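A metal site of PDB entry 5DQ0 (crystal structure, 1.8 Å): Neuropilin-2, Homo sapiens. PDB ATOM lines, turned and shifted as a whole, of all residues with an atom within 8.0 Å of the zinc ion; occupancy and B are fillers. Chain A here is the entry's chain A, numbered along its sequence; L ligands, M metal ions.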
ATOM      1  N   LEU A  92       4.661 -11.887  22.877  1.00  0.00           N
ATOM      2  CA  LEU A  92       3.527 -12.576  22.360  1.00  0.00           C
ATOM      3  C   LEU A  92       2.882 -11.673  21.317  1.00  0.00           C
ATOM      4  O   LEU A  92       2.708 -10.492  21.582  1.00  0.00           O
ATOM      5  CB  LEU A  92       2.543 -12.826  23.484  1.00  0.00           C
ATOM      6  CG  LEU A  92       1.126 -13.263  23.239  1.00  0.00           C
ATOM      7  CD1 LEU A  92       1.036 -14.659  22.644  1.00  0.00           C
ATOM      8  CD2 LEU A  92       0.293 -13.150  24.509  1.00  0.00           C
ATOM      9  N   TYR A 104       1.410  -8.026  22.161  1.00  0.00           N
ATOM     10  CA  TYR A 104       0.729  -7.899  23.433  1.00  0.00           C
ATOM     11  C   TYR A 104       1.491  -6.914  24.352  1.00  0.00           C
ATOM     12  O   TYR A 104       2.714  -7.047  24.520  1.00  0.00           O
ATOM     13  CB  TYR A 104       0.574  -9.251  24.124  1.00  0.00           C
ATOM     14  CG  TYR A 104      -0.118  -9.178  25.481  1.00  0.00           C
ATOM     15  CD1 TYR A 104      -1.402  -8.687  25.608  1.00  0.00           C
ATOM     16  CD2 TYR A 104       0.516  -9.597  26.636  1.00  0.00           C
ATOM     17  CE1 TYR A 104      -2.026  -8.598  26.854  1.00  0.00           C
ATOM     18  CE2 TYR A 104      -0.083  -9.503  27.907  1.00  0.00           C
ATOM     19  CZ  TYR A 104      -1.362  -9.008  28.013  1.00  0.00           C
ATOM     20  OH  TYR A 104      -2.034  -8.921  29.224  1.00  0.00           O
ATOM     21  N   ARG A 105       0.750  -5.934  24.857  1.00  0.00           N
ATOM     22  CA  ARG A 105       1.353  -4.844  25.660  1.00  0.00           C
ATOM     23  C   ARG A 105       0.572  -4.574  26.922  1.00  0.00           C
ATOM     24  O   ARG A 105      -0.587  -4.893  27.054  1.00  0.00           O
ATOM     25  CB  ARG A 105       1.537  -3.534  24.893  1.00  0.00           C
ATOM     26  CG  ARG A 105       0.491  -3.166  23.938  1.00  0.00           C
ATOM     27  CD  ARG A 105       0.895  -1.915  23.146  1.00  0.00           C
ATOM     28  NE  ARG A 105      -0.362  -1.363  22.655  1.00  0.00           N
ATOM     29  CZ  ARG A 105      -0.934  -1.660  21.484  1.00  0.00           C
ATOM     30  NH1 ARG A 105      -0.358  -2.479  20.577  1.00  0.00           N
ATOM     31  NH2 ARG A 105      -2.102  -1.091  21.191  1.00  0.00           N
ATOM     32  N   HIS A 106       1.275  -3.964  27.874  1.00  0.00           N
ATOM     33  CA  HIS A 106       0.682  -3.296  29.017  1.00  0.00           C
ATOM     34  C   HIS A 106       0.930  -1.792  28.792  1.00  0.00           C
ATOM     35  O   HIS A 106       2.103  -1.372  28.750  1.00  0.00           O
ATOM     36  CB  HIS A 106       1.422  -3.768  30.277  1.00  0.00           C
ATOM     37  CG  HIS A 106       1.120  -5.165  30.670  1.00  0.00           C
ATOM     38  ND1 HIS A 106       1.751  -5.762  31.733  1.00  0.00           N
ATOM     39  CD2 HIS A 106       0.213  -6.072  30.215  1.00  0.00           C
ATOM     40  CE1 HIS A 106       1.251  -6.980  31.918  1.00  0.00           C
ATOM     41  NE2 HIS A 106       0.332  -7.187  31.000  1.00  0.00           N
ATOM     42  N   LYS A 111       4.742  -6.522  26.527  1.00  0.00           N
ATOM     43  CA  LYS A 111       4.945  -7.432  27.644  1.00  0.00           C
ATOM     44  C   LYS A 111       6.044  -8.423  27.331  1.00  0.00           C
ATOM     45  O   LYS A 111       5.976  -9.165  26.360  1.00  0.00           O
ATOM     46  CB  LYS A 111       3.617  -8.083  27.997  1.00  0.00           C
ATOM     47  CG  LYS A 111       3.705  -9.145  29.080  1.00  0.00           C
ATOM     48  CD  LYS A 111       4.227  -8.649  30.419  1.00  0.00           C
ATOM     49  CE  LYS A 111       4.305  -9.843  31.418  1.00  0.00           C
ATOM     50  NZ  LYS A 111       4.801  -9.351  32.732  1.00  0.00           N
ATOM     51  N   PHE A 113       7.650 -11.689  28.605  1.00  0.00           N
ATOM     52  CA  PHE A 113       7.464 -12.799  29.538  1.00  0.00           C
ATOM     53  C   PHE A 113       8.832 -13.411  29.866  1.00  0.00           C
ATOM     54  O   PHE A 113       9.606 -13.697  28.987  1.00  0.00           O
ATOM     55  CB  PHE A 113       6.517 -13.855  28.940  1.00  0.00           C
ATOM     56  CG  PHE A 113       5.118 -13.344  28.739  1.00  0.00           C
ATOM     57  CD1 PHE A 113       4.167 -13.476  29.736  1.00  0.00           C
ATOM     58  CD2 PHE A 113       4.725 -12.820  27.522  1.00  0.00           C
ATOM     59  CE1 PHE A 113       2.866 -13.074  29.556  1.00  0.00           C
ATOM     60  CE2 PHE A 113       3.417 -12.352  27.349  1.00  0.00           C
ATOM     61  CZ  PHE A 113       2.496 -12.475  28.350  1.00  0.00           C
ATOM     62  N   LYS A 126       0.896 -16.895  33.712  1.00  0.00           N
ATOM     63  CA  LYS A 126      -0.512 -16.576  33.625  1.00  0.00           C
ATOM     64  C   LYS A 126      -0.671 -15.123  33.146  1.00  0.00           C
ATOM     65  O   LYS A 126       0.046 -14.253  33.610  1.00  0.00           O
ATOM     66  CB  LYS A 126      -1.207 -16.782  34.968  1.00  0.00           C
ATOM     67  CG  LYS A 126      -1.087 -18.224  35.468  1.00  0.00           C
ATOM     68  CD  LYS A 126      -1.811 -18.422  36.805  1.00  0.00           C
ATOM     69  CE  LYS A 126      -1.836 -19.906  37.201  1.00  0.00           C
ATOM     70  NZ  LYS A 126      -2.152 -20.083  38.640  1.00  0.00           N
ATOM     71  N   LEU A 127      -1.600 -14.852  32.242  1.00  0.00           N
ATOM     72  CA  LEU A 127      -1.888 -13.475  31.839  1.00  0.00           C
ATOM     73  C   LEU A 127      -2.693 -12.764  32.912  1.00  0.00           C
ATOM     74  O   LEU A 127      -3.534 -13.364  33.574  1.00  0.00           O
ATOM     75  CB  LEU A 127      -2.630 -13.453  30.513  1.00  0.00           C
ATOM     76  CG  LEU A 127      -1.730 -13.561  29.255  1.00  0.00           C
ATOM     77  CD1 LEU A 127      -1.057 -14.905  29.124  1.00  0.00           C
ATOM     78  CD2 LEU A 127      -2.623 -13.377  28.065  1.00  0.00           C
ATOM     79  N   HIS A 128      -2.517 -11.451  33.044  1.00  0.00           N
ATOM     80  CA  HIS A 128      -3.189 -10.713  34.117  1.00  0.00           C
ATOM     81  C   HIS A 128      -4.681 -10.651  33.926  1.00  0.00           C
ATOM     82  O   HIS A 128      -5.425 -10.446  34.894  1.00  0.00           O
ATOM     83  CB  HIS A 128      -2.579  -9.312  34.262  1.00  0.00           C
ATOM     84  CG  HIS A 128      -3.145  -8.320  33.322  1.00  0.00           C
ATOM     85  ND1 HIS A 128      -2.700  -8.160  32.031  1.00  0.00           N
ATOM     86  CD2 HIS A 128      -4.167  -7.443  33.486  1.00  0.00           C
ATOM     87  CE1 HIS A 128      -3.434  -7.239  31.435  1.00  0.00           C
ATOM     88  NE2 HIS A 128      -4.326  -6.778  32.301  1.00  0.00           N
ATOM     89  N   ALA A 129      -5.133 -10.767  32.688  1.00  0.00           N
ATOM     90  CA  ALA A 129      -6.525 -10.874  32.347  1.00  0.00           C
ATOM     91  C   ALA A 129      -6.633 -11.638  31.053  1.00  0.00           C
ATOM     92  O   ALA A 129      -5.692 -11.704  30.287  1.00  0.00           O
ATOM     93  CB  ALA A 129      -7.166  -9.487  32.217  1.00  0.00           C
ATOM     94  N   PRO A 130      -7.773 -12.274  30.798  1.00  0.00           N
ATOM     95  CA  PRO A 130      -7.812 -13.082  29.592  1.00  0.00           C
ATOM     96  C   PRO A 130      -7.719 -12.217  28.288  1.00  0.00           C
ATOM     97  O   PRO A 130      -8.147 -11.064  28.247  1.00  0.00           O
ATOM     98  CB  PRO A 130      -9.150 -13.777  29.713  1.00  0.00           C
ATOM     99  CG  PRO A 130      -9.550 -13.690  31.161  1.00  0.00           C
ATOM    100  CD  PRO A 130      -9.009 -12.384  31.594  1.00  0.00           C
ATOM    101  N   LEU A 131      -7.044 -12.771  27.299  1.00  0.00           N
ATOM    102  CA  LEU A 131      -6.743 -12.047  26.073  1.00  0.00           C
ATOM    103  C   LEU A 131      -7.444 -12.731  24.906  1.00  0.00           C
ATOM    104  O   LEU A 131      -7.262 -13.933  24.723  1.00  0.00           O
ATOM    105  CB  LEU A 131      -5.249 -12.069  25.883  1.00  0.00           C
ATOM    106  CG  LEU A 131      -4.613 -11.588  24.567  1.00  0.00           C
ATOM    107  CD1 LEU A 131      -5.026 -10.130  24.366  1.00  0.00           C
ATOM    108  CD2 LEU A 131      -3.092 -11.760  24.565  1.00  0.00           C
HETATM  109 CL1  LIG L   1       0.110 -10.421  31.565  1.00  0.00          CL
HETATM  110 ZN    ZN M   1      -1.071  -8.777  30.875  1.00  0.00          ZN
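The backbone carbonyl oxygen of Tyr 104 lies within hydrogen-bond range of the backbone NH of Lys 111.
The backbone NH (N) of Tyr 104 sits at hydrogen-bond distance from the backbone carbonyl oxygen (O) of Leu 92 (2.8 Å).
The zinc ion is bound by the side-chain hydroxyl of Tyr 104 (1.9 Å), a ring nitrogen (ND1) of His 128 (2.1 Å), a ring nitrogen (NE2) of His 106 (2.1 Å) and a chlorine (CL1) of the ligand (2.1 Å).
The zinc ion has four donor atoms within binding distance.
Within 4 Å of the zinc ion: Tyr 104, His 106 and His 128.
Along chain A the residues within 4 Å of the zinc ion span positions 104 to 128.
The nearest printed residue that does not touch the zinc ion is Leu 127 (4.8 Å).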
